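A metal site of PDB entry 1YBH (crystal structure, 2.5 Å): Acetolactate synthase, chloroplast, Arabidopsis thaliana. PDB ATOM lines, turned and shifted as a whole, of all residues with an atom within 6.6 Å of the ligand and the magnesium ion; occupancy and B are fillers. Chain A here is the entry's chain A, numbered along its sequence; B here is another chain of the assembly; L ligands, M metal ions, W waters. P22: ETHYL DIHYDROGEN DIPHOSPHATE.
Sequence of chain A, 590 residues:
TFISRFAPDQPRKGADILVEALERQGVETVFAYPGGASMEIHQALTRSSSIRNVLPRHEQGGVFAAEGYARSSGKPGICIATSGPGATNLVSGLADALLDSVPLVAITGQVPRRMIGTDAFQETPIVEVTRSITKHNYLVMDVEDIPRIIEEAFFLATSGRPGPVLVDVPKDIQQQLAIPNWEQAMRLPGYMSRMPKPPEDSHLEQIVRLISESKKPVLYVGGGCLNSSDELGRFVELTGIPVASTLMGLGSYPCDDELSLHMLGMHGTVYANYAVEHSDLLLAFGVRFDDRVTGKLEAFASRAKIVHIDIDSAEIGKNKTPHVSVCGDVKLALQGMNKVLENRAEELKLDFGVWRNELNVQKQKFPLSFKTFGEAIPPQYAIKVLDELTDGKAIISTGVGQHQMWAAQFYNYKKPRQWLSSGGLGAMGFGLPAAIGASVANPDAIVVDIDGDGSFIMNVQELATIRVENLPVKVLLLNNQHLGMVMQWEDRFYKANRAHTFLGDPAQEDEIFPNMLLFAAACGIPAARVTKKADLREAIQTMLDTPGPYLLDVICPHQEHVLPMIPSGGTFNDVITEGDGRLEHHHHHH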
ATOM      1  N   GLY A 399       0.573 -11.521  32.384  1.00  0.00           N
ATOM      2  CA  GLY A 399       0.869 -12.705  31.601  1.00  0.00           C
ATOM      3  C   GLY A 399       1.397 -12.147  30.297  1.00  0.00           C
ATOM      4  O   GLY A 399       1.906 -11.033  30.256  1.00  0.00           O
ATOM      5  N   VAL A 400       1.263 -12.917  29.229  1.00  0.00           N
ATOM      6  CA  VAL A 400       1.736 -12.471  27.914  1.00  0.00           C
ATOM      7  C   VAL A 400       0.599 -12.494  26.903  1.00  0.00           C
ATOM      8  O   VAL A 400      -0.177 -13.447  26.864  1.00  0.00           O
ATOM      9  CB  VAL A 400       2.892 -13.376  27.405  1.00  0.00           C
ATOM     10  CG1 VAL A 400       3.182 -13.081  25.954  1.00  0.00           C
ATOM     11  CG2 VAL A 400       4.130 -13.136  28.246  1.00  0.00           C
ATOM     12  N   GLY A 401       0.497 -11.447  26.103  1.00  0.00           N
ATOM     13  CA  GLY A 401      -0.558 -11.387  25.102  1.00  0.00           C
ATOM     14  C   GLY A 401      -1.215 -10.021  25.036  1.00  0.00           C
ATOM     15  O   GLY A 401      -0.603  -9.002  25.382  1.00  0.00           O
ATOM     16  N   GLN A 402      -2.467  -9.991  24.593  1.00  0.00           N
ATOM     17  CA  GLN A 402      -3.213  -8.743  24.478  1.00  0.00           C
ATOM     18  C   GLN A 402      -3.330  -8.014  25.818  1.00  0.00           C
ATOM     19  O   GLN A 402      -3.067  -6.812  25.885  1.00  0.00           O
ATOM     20  CB  GLN A 402      -4.605  -8.991  23.925  1.00  0.00           C
ATOM     21  CG  GLN A 402      -4.639  -9.548  22.512  1.00  0.00           C
ATOM     22  CD  GLN A 402      -6.051  -9.671  21.988  1.00  0.00           C
ATOM     23  OE1 GLN A 402      -6.926 -10.240  22.655  1.00  0.00           O
ATOM     24  NE2 GLN A 402      -6.301  -9.146  20.795  1.00  0.00           N
ATOM     25  N   HIS A 403      -3.732  -8.731  26.864  1.00  0.00           N
ATOM     26  CA  HIS A 403      -3.878  -8.107  28.173  1.00  0.00           C
ATOM     27  C   HIS A 403      -2.572  -7.440  28.615  1.00  0.00           C
ATOM     28  O   HIS A 403      -2.585  -6.377  29.260  1.00  0.00           O
ATOM     29  CB  HIS A 403      -4.335  -9.115  29.233  1.00  0.00           C
ATOM     30  CG  HIS A 403      -3.311 -10.143  29.618  1.00  0.00           C
ATOM     31  ND1 HIS A 403      -2.993 -11.218  28.823  1.00  0.00           N
ATOM     32  CD2 HIS A 403      -2.554 -10.266  30.734  1.00  0.00           C
ATOM     33  CE1 HIS A 403      -2.097 -11.970  29.435  1.00  0.00           C
ATOM     34  NE2 HIS A 403      -1.810 -11.420  30.597  1.00  0.00           N
ATOM     35  N   GLN A 404      -1.452  -8.043  28.235  1.00  0.00           N
ATOM     36  CA  GLN A 404      -0.151  -7.511  28.582  1.00  0.00           C
ATOM     37  C   GLN A 404       0.017  -6.155  27.896  1.00  0.00           C
ATOM     38  O   GLN A 404       0.422  -5.167  28.519  1.00  0.00           O
ATOM     39  CB  GLN A 404       0.942  -8.487  28.137  1.00  0.00           C
ATOM     40  CG  GLN A 404       2.369  -8.017  28.334  1.00  0.00           C
ATOM     41  CD  GLN A 404       3.365  -9.018  27.786  1.00  0.00           C
ATOM     42  OE1 GLN A 404       3.107  -9.679  26.773  1.00  0.00           O
ATOM     43  NE2 GLN A 404       4.527  -9.129  28.436  1.00  0.00           N
ATOM     44  N   TRP A 406      -2.335  -4.208  26.859  1.00  0.00           N
ATOM     45  CA  TRP A 406      -3.255  -3.253  27.444  1.00  0.00           C
ATOM     46  C   TRP A 406      -2.793  -2.822  28.826  1.00  0.00           C
ATOM     47  O   TRP A 406      -2.956  -1.658  29.185  1.00  0.00           O
ATOM     48  CB  TRP A 406      -4.680  -3.827  27.501  1.00  0.00           C
ATOM     49  CG  TRP A 406      -5.290  -3.983  26.133  1.00  0.00           C
ATOM     50  CD1 TRP A 406      -5.166  -3.115  25.075  1.00  0.00           C
ATOM     51  CD2 TRP A 406      -6.059  -5.088  25.672  1.00  0.00           C
ATOM     52  NE1 TRP A 406      -5.808  -3.636  23.975  1.00  0.00           N
ATOM     53  CE2 TRP A 406      -6.371  -4.839  24.313  1.00  0.00           C
ATOM     54  CE3 TRP A 406      -6.524  -6.274  26.267  1.00  0.00           C
ATOM     55  CZ2 TRP A 406      -7.113  -5.737  23.543  1.00  0.00           C
ATOM     56  CZ3 TRP A 406      -7.257  -7.161  25.502  1.00  0.00           C
ATOM     57  CH2 TRP A 406      -7.553  -6.891  24.151  1.00  0.00           C
ATOM     58  N   MET A 428       4.239 -17.130  29.070  1.00  0.00           N
ATOM     59  CA  MET A 428       2.929 -17.147  29.701  1.00  0.00           C
ATOM     60  C   MET A 428       3.039 -17.808  31.073  1.00  0.00           C
ATOM     61  O   MET A 428       3.960 -18.594  31.310  1.00  0.00           O
ATOM     62  CB  MET A 428       1.944 -17.938  28.826  1.00  0.00           C
ATOM     63  CG  MET A 428       1.427 -17.180  27.629  1.00  0.00           C
ATOM     64  SD  MET A 428       0.481 -18.253  26.549  1.00  0.00           S
ATOM     65  CE  MET A 428      -0.986 -18.551  27.543  1.00  0.00           C
ATOM     66  N   ASP A 451      -3.876 -10.671  34.564  1.00  0.00           N
ATOM     67  CA  ASP A 451      -3.661 -11.876  33.775  1.00  0.00           C
ATOM     68  C   ASP A 451      -4.672 -12.147  32.656  1.00  0.00           C
ATOM     69  O   ASP A 451      -5.697 -11.493  32.549  1.00  0.00           O
ATOM     70  CB  ASP A 451      -3.655 -13.084  34.715  1.00  0.00           C
ATOM     71  CG  ASP A 451      -2.439 -13.972  34.534  1.00  0.00           C
ATOM     72  OD1 ASP A 451      -1.967 -14.128  33.394  1.00  0.00           O
ATOM     73  OD2 ASP A 451      -1.966 -14.523  35.556  1.00  0.00           O
ATOM     74  N   GLY A 452      -4.336 -13.136  31.824  1.00  0.00           N
ATOM     75  CA  GLY A 452      -5.175 -13.555  30.726  1.00  0.00           C
ATOM     76  C   GLY A 452      -5.653 -14.939  31.142  1.00  0.00           C
ATOM     77  O   GLY A 452      -4.980 -15.582  31.949  1.00  0.00           O
ATOM     78  N   ASP A 453      -6.775 -15.408  30.605  1.00  0.00           N
ATOM     79  CA  ASP A 453      -7.280 -16.712  31.013  1.00  0.00           C
ATOM     80  C   ASP A 453      -6.370 -17.839  30.569  1.00  0.00           C
ATOM     81  O   ASP A 453      -6.299 -18.877  31.221  1.00  0.00           O
ATOM     82  CB  ASP A 453      -8.721 -16.943  30.509  1.00  0.00           C
ATOM     83  CG  ASP A 453      -8.847 -16.828  28.993  1.00  0.00           C
ATOM     84  OD1 ASP A 453      -8.550 -15.747  28.441  1.00  0.00           O
ATOM     85  OD2 ASP A 453      -9.254 -17.828  28.357  1.00  0.00           O
ATOM     86  N   GLY A 454      -5.646 -17.635  29.473  1.00  0.00           N
ATOM     87  CA  GLY A 454      -4.729 -18.664  29.007  1.00  0.00           C
ATOM     88  C   GLY A 454      -3.485 -18.691  29.892  1.00  0.00           C
ATOM     89  O   GLY A 454      -3.071 -19.756  30.361  1.00  0.00           O
ATOM     90  N   SER A 455      -2.914 -17.515  30.136  1.00  0.00           N
ATOM     91  CA  SER A 455      -1.717 -17.399  30.964  1.00  0.00           C
ATOM     92  C   SER A 455      -1.980 -17.744  32.418  1.00  0.00           C
ATOM     93  O   SER A 455      -1.169 -18.400  33.066  1.00  0.00           O
ATOM     94  CB  SER A 455      -1.159 -15.973  30.913  1.00  0.00           C
ATOM     95  OG  SER A 455      -0.846 -15.588  29.591  1.00  0.00           O
ATOM     96  N   PHE A 456      -3.126 -17.294  32.925  1.00  0.00           N
ATOM     97  CA  PHE A 456      -3.475 -17.528  34.312  1.00  0.00           C
ATOM     98  C   PHE A 456      -3.590 -19.010  34.681  1.00  0.00           C
ATOM     99  O   PHE A 456      -3.121 -19.424  35.742  1.00  0.00           O
ATOM    100  CB  PHE A 456      -4.793 -16.830  34.645  1.00  0.00           C
ATOM    101  CG  PHE A 456      -5.268 -17.071  36.054  1.00  0.00           C
ATOM    102  CD1 PHE A 456      -4.678 -16.393  37.118  1.00  0.00           C
ATOM    103  CD2 PHE A 456      -6.294 -17.979  36.324  1.00  0.00           C
ATOM    104  CE1 PHE A 456      -5.103 -16.626  38.438  1.00  0.00           C
ATOM    105  CE2 PHE A 456      -6.720 -18.224  37.631  1.00  0.00           C
ATOM    106  CZ  PHE A 456      -6.117 -17.547  38.693  1.00  0.00           C
ATOM    107  N   LEU A 478      -8.474 -10.704  32.929  1.00  0.00           N
ATOM    108  CA  LEU A 478      -9.204 -10.257  31.747  1.00  0.00           C
ATOM    109  C   LEU A 478      -9.516 -11.514  30.944  1.00  0.00           C
ATOM    110  O   LEU A 478      -8.740 -11.932  30.087  1.00  0.00           O
ATOM    111  CB  LEU A 478      -8.367  -9.287  30.919  1.00  0.00           C
ATOM    112  CG  LEU A 478      -7.954  -8.026  31.683  1.00  0.00           C
ATOM    113  CD1 LEU A 478      -7.249  -7.041  30.745  1.00  0.00           C
ATOM    114  CD2 LEU A 478      -9.185  -7.388  32.301  1.00  0.00           C
ATOM    115  N   ASN A 479     -10.663 -12.113  31.255  1.00  0.00           N
ATOM    116  CA  ASN A 479     -11.092 -13.356  30.614  1.00  0.00           C
ATOM    117  C   ASN A 479     -11.782 -13.144  29.271  1.00  0.00           C
ATOM    118  O   ASN A 479     -12.844 -12.525  29.205  1.00  0.00           O
ATOM    119  CB  ASN A 479     -12.026 -14.096  31.562  1.00  0.00           C
ATOM    120  CG  ASN A 479     -12.218 -15.546  31.172  1.00  0.00           C
ATOM    121  OD1 ASN A 479     -12.072 -15.918  30.000  1.00  0.00           O
ATOM    122  ND2 ASN A 479     -12.562 -16.374  32.151  1.00  0.00           N
ATOM    123  N   ASN A 480     -11.187 -13.664  28.199  1.00  0.00           N
ATOM    124  CA  ASN A 480     -11.778 -13.541  26.867  1.00  0.00           C
ATOM    125  C   ASN A 480     -11.921 -14.902  26.189  1.00  0.00           C
ATOM    126  O   ASN A 480     -12.139 -14.984  24.984  1.00  0.00           O
ATOM    127  CB  ASN A 480     -10.939 -12.587  26.005  1.00  0.00           C
ATOM    128  CG  ASN A 480      -9.585 -13.183  25.608  1.00  0.00           C
ATOM    129  OD1 ASN A 480      -9.162 -14.220  26.129  1.00  0.00           O
ATOM    130  ND2 ASN A 480      -8.905 -12.507  24.697  1.00  0.00           N
ATOM    131  N   GLN A 481     -11.786 -15.970  26.979  1.00  0.00           N
ATOM    132  CA  GLN A 481     -11.938 -17.327  26.468  1.00  0.00           C
ATOM    133  C   GLN A 481     -11.032 -17.719  25.304  1.00  0.00           C
ATOM    134  O   GLN A 481     -11.196 -18.793  24.719  1.00  0.00           O
ATOM    135  CB  GLN A 481     -13.385 -17.544  26.057  1.00  0.00           C
ATOM    136  CG  GLN A 481     -14.383 -17.302  27.163  1.00  0.00           C
ATOM    137  CD  GLN A 481     -14.306 -18.356  28.258  1.00  0.00           C
ATOM    138  OE1 GLN A 481     -13.496 -18.255  29.181  1.00  0.00           O
ATOM    139  NE2 GLN A 481     -15.145 -19.381  28.145  1.00  0.00           N
ATOM    140  N   HIS A 482     -10.078 -16.863  24.952  1.00  0.00           N
ATOM    141  CA  HIS A 482      -9.166 -17.165  23.854  1.00  0.00           C
ATOM    142  C   HIS A 482      -7.699 -16.862  24.155  1.00  0.00           C
ATOM    143  O   HIS A 482      -7.344 -16.337  25.208  1.00  0.00           O
ATOM    144  CB  HIS A 482      -9.532 -16.333  22.607  1.00  0.00           C
ATOM    145  CG  HIS A 482     -10.809 -16.749  21.950  1.00  0.00           C
ATOM    146  ND1 HIS A 482     -12.045 -16.533  22.513  1.00  0.00           N
ATOM    147  CD2 HIS A 482     -11.038 -17.346  20.749  1.00  0.00           C
ATOM    148  CE1 HIS A 482     -12.983 -16.982  21.697  1.00  0.00           C
ATOM    149  NE2 HIS A 482     -12.402 -17.492  20.626  1.00  0.00           N
ATOM    150  N   LEU A 483      -6.853 -17.235  23.194  1.00  0.00           N
ATOM    151  CA  LEU A 483      -5.438 -16.936  23.258  1.00  0.00           C
ATOM    152  C   LEU A 483      -5.438 -15.687  22.391  1.00  0.00           C
ATOM    153  O   LEU A 483      -5.120 -15.717  21.207  1.00  0.00           O
ATOM    154  CB  LEU A 483      -4.609 -18.051  22.616  1.00  0.00           C
ATOM    155  CG  LEU A 483      -4.609 -19.371  23.407  1.00  0.00           C
ATOM    156  CD1 LEU A 483      -3.832 -20.451  22.660  1.00  0.00           C
ATOM    157  CD2 LEU A 483      -4.004 -19.135  24.772  1.00  0.00           C
ATOM    158  N   GLY A 484      -5.852 -14.584  23.024  1.00  0.00           N
ATOM    159  CA  GLY A 484      -5.982 -13.294  22.368  1.00  0.00           C
ATOM    160  C   GLY A 484      -5.023 -12.878  21.274  1.00  0.00           C
ATOM    161  O   GLY A 484      -5.447 -12.585  20.151  1.00  0.00           O
ATOM    162  N   MET A 485      -3.730 -12.815  21.595  1.00  0.00           N
ATOM    163  CA  MET A 485      -2.734 -12.379  20.638  1.00  0.00           C
ATOM    164  C   MET A 485      -2.662 -13.275  19.402  1.00  0.00           C
ATOM    165  O   MET A 485      -2.593 -12.770  18.282  1.00  0.00           O
ATOM    166  CB  MET A 485      -1.363 -12.285  21.311  1.00  0.00           C
ATOM    167  CG  MET A 485      -0.291 -11.601  20.472  1.00  0.00           C
ATOM    168  SD  MET A 485      -0.760  -9.935  19.962  1.00  0.00           S
ATOM    169  CE  MET A 485      -0.443  -9.020  21.479  1.00  0.00           C
ATOM    170  N   VAL A 486      -2.687 -14.592  19.588  1.00  0.00           N
ATOM    171  CA  VAL A 486      -2.621 -15.504  18.449  1.00  0.00           C
ATOM    172  C   VAL A 486      -3.870 -15.341  17.603  1.00  0.00           C
ATOM    173  O   VAL A 486      -3.834 -15.417  16.370  1.00  0.00           O
ATOM    174  CB  VAL A 486      -2.524 -16.968  18.882  1.00  0.00           C
ATOM    175  CG1 VAL A 486      -2.420 -17.880  17.672  1.00  0.00           C
ATOM    176  CG2 VAL A 486      -1.326 -17.156  19.769  1.00  0.00           C
ATOM    177  N   LEU A 503     -10.091 -21.257  24.189  1.00  0.00           N
ATOM    178  CA  LEU A 503      -9.830 -21.911  25.471  1.00  0.00           C
ATOM    179  C   LEU A 503     -11.062 -22.427  26.218  1.00  0.00           C
ATOM    180  O   LEU A 503     -10.922 -23.098  27.240  1.00  0.00           O
ATOM    181  CB  LEU A 503      -9.069 -20.941  26.393  1.00  0.00           C
ATOM    182  CG  LEU A 503      -7.704 -20.490  25.901  1.00  0.00           C
ATOM    183  CD1 LEU A 503      -7.181 -19.372  26.791  1.00  0.00           C
ATOM    184  CD2 LEU A 503      -6.750 -21.668  25.870  1.00  0.00           C
ATOM    185  N   TYR B  33       0.258 -26.704  21.331  1.00  0.00           N
ATOM    186  CA  TYR B  33      -0.191 -25.448  21.905  1.00  0.00           C
ATOM    187  C   TYR B  33       0.369 -24.360  20.983  1.00  0.00           C
ATOM    188  O   TYR B  33       1.582 -24.175  20.880  1.00  0.00           O
ATOM    189  CB  TYR B  33       0.377 -25.286  23.315  1.00  0.00           C
ATOM    190  CG  TYR B  33      -0.325 -24.247  24.135  1.00  0.00           C
ATOM    191  CD1 TYR B  33      -1.397 -24.570  24.959  1.00  0.00           C
ATOM    192  CD2 TYR B  33       0.073 -22.912  24.080  1.00  0.00           C
ATOM    193  CE1 TYR B  33      -2.062 -23.593  25.702  1.00  0.00           C
ATOM    194  CE2 TYR B  33      -0.578 -21.935  24.821  1.00  0.00           C
ATOM    195  CZ  TYR B  33      -1.639 -22.280  25.632  1.00  0.00           C
ATOM    196  OH  TYR B  33      -2.281 -21.297  26.341  1.00  0.00           O
ATOM    197  N   PRO B  34      -0.510 -23.628  20.299  1.00  0.00           N
ATOM    198  CA  PRO B  34      -0.147 -22.562  19.362  1.00  0.00           C
ATOM    199  C   PRO B  34       0.595 -21.377  19.952  1.00  0.00           C
ATOM    200  O   PRO B  34       0.356 -20.962  21.075  1.00  0.00           O
ATOM    201  CB  PRO B  34      -1.490 -22.147  18.784  1.00  0.00           C
ATOM    202  CG  PRO B  34      -2.376 -22.276  19.977  1.00  0.00           C
ATOM    203  CD  PRO B  34      -1.966 -23.608  20.557  1.00  0.00           C
HETATM  204  C6  P22 L   1      -1.345 -15.704  23.877  1.00  0.00           C
HETATM  205  C7  P22 L   1      -2.026 -15.541  25.276  1.00  0.00           C
HETATM  206  O7  P22 L   1      -3.252 -15.952  25.913  1.00  0.00           O
HETATM  207  PA  P22 L   1      -3.951 -15.156  27.144  1.00  0.00           P
HETATM  208  O1A P22 L   1      -5.317 -15.599  27.273  1.00  0.00           O
HETATM  209  O2A P22 L   1      -3.287 -15.415  28.375  1.00  0.00           O
HETATM  210  O3A P22 L   1      -4.022 -13.585  26.900  1.00  0.00           O
HETATM  211  PB  P22 L   1      -4.576 -12.591  25.792  1.00  0.00           P
HETATM  212  O1B P22 L   1      -3.604 -12.549  24.699  1.00  0.00           O
HETATM  213  O2B P22 L   1      -4.729 -11.379  26.562  1.00  0.00           O
HETATM  214  O3B P22 L   1      -5.869 -13.212  25.464  1.00  0.00           O
HETATM  215 MG    MG M   1      -7.034 -14.715  26.791  1.00  0.00          MG
HETATM  216  O   HOH W   1      -7.258 -13.062  28.790  1.00  0.00           O
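Merely in contact with the ligand: Val 400 (3.2 Å), Gly 401 (3.3 Å), Met 428 (3.8 Å), Gly 452 (3.5 Å) and Leu 483 (3.5 Å).
Hydrophobic or aromatic side chains that line the ligand: His 403, Met 428 and Leu 483.
Of the 26 residues printed, 14 come within 4 Å of the ligand.
The nearest printed residue that does not touch the ligand is Leu 503 (4.2 Å).
The magnesium ion is bound by an oxygen (O1A) of the ligand (2.0 Å), the side-chain amide oxygen of Asn 480 (2.3 Å), the backbone carbonyl oxygen of His 482 (2.3 Å), an oxygen (O3B) of the ligand (2.3 Å) and the side-chain carboxylate of Asp 453 (2.5 Å).
The magnesium ion has five donor atoms within binding distance.
Slightly farther from the magnesium ion lies water W1 (2.6 Å).
An oxygen (O2A) of the ligand lies within hydrogen-bond range of the backbone NH (N) of Ser 455 (2.8 Å).
An oxygen (O2A) of the ligand lies within hydrogen-bond range of the side-chain hydroxyl of Ser 455, at 2.7 Å.
The backbone NH of Gly 484 lies close to an oxygen (O1B) of the ligand (3.5 Å).
O1B of the ligand is in hydrogen-bond range of N of Gln 402, at 2.8 Å.
N of His 403 sits at hydrogen-bond distance from O2B of the ligand, at 2.8 Å.
An oxygen (O2B) of the ligand is in hydrogen-bond range of a ring nitrogen (ND1) of His 403, at 2.9 Å.
N of Gly 454 sits at hydrogen-bond distance from O2A of the ligand.
O1B of the ligand lies within hydrogen-bond range of N of Met 485 (3.1 Å).
The side-chain carboxylate (OD2) of Asp 453 lies close to the backbone NH (N) of Gln 481 (3.4 Å).
The side-chain hydroxyl of Ser 455 is in hydrogen-bond range of the backbone NH of Val 400 (3.4 Å).
A ring nitrogen (NE2) of His 403 sits at hydrogen-bond distance from the backbone NH of Gly 452, 3.3 Å away.
N of Gly 399 sits at hydrogen-bond distance from NE2 of His 403 (3.0 Å).
The backbone NH of Gly 401 lies within hydrogen-bond range of the side-chain amide oxygen of Gln 404.
Residues that only touch the magnesium ion: Gly 484 (3.95 Å).
Within 4 Å of the magnesium ion: Asp 453, Asn 480, His 482 and Gly 484.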
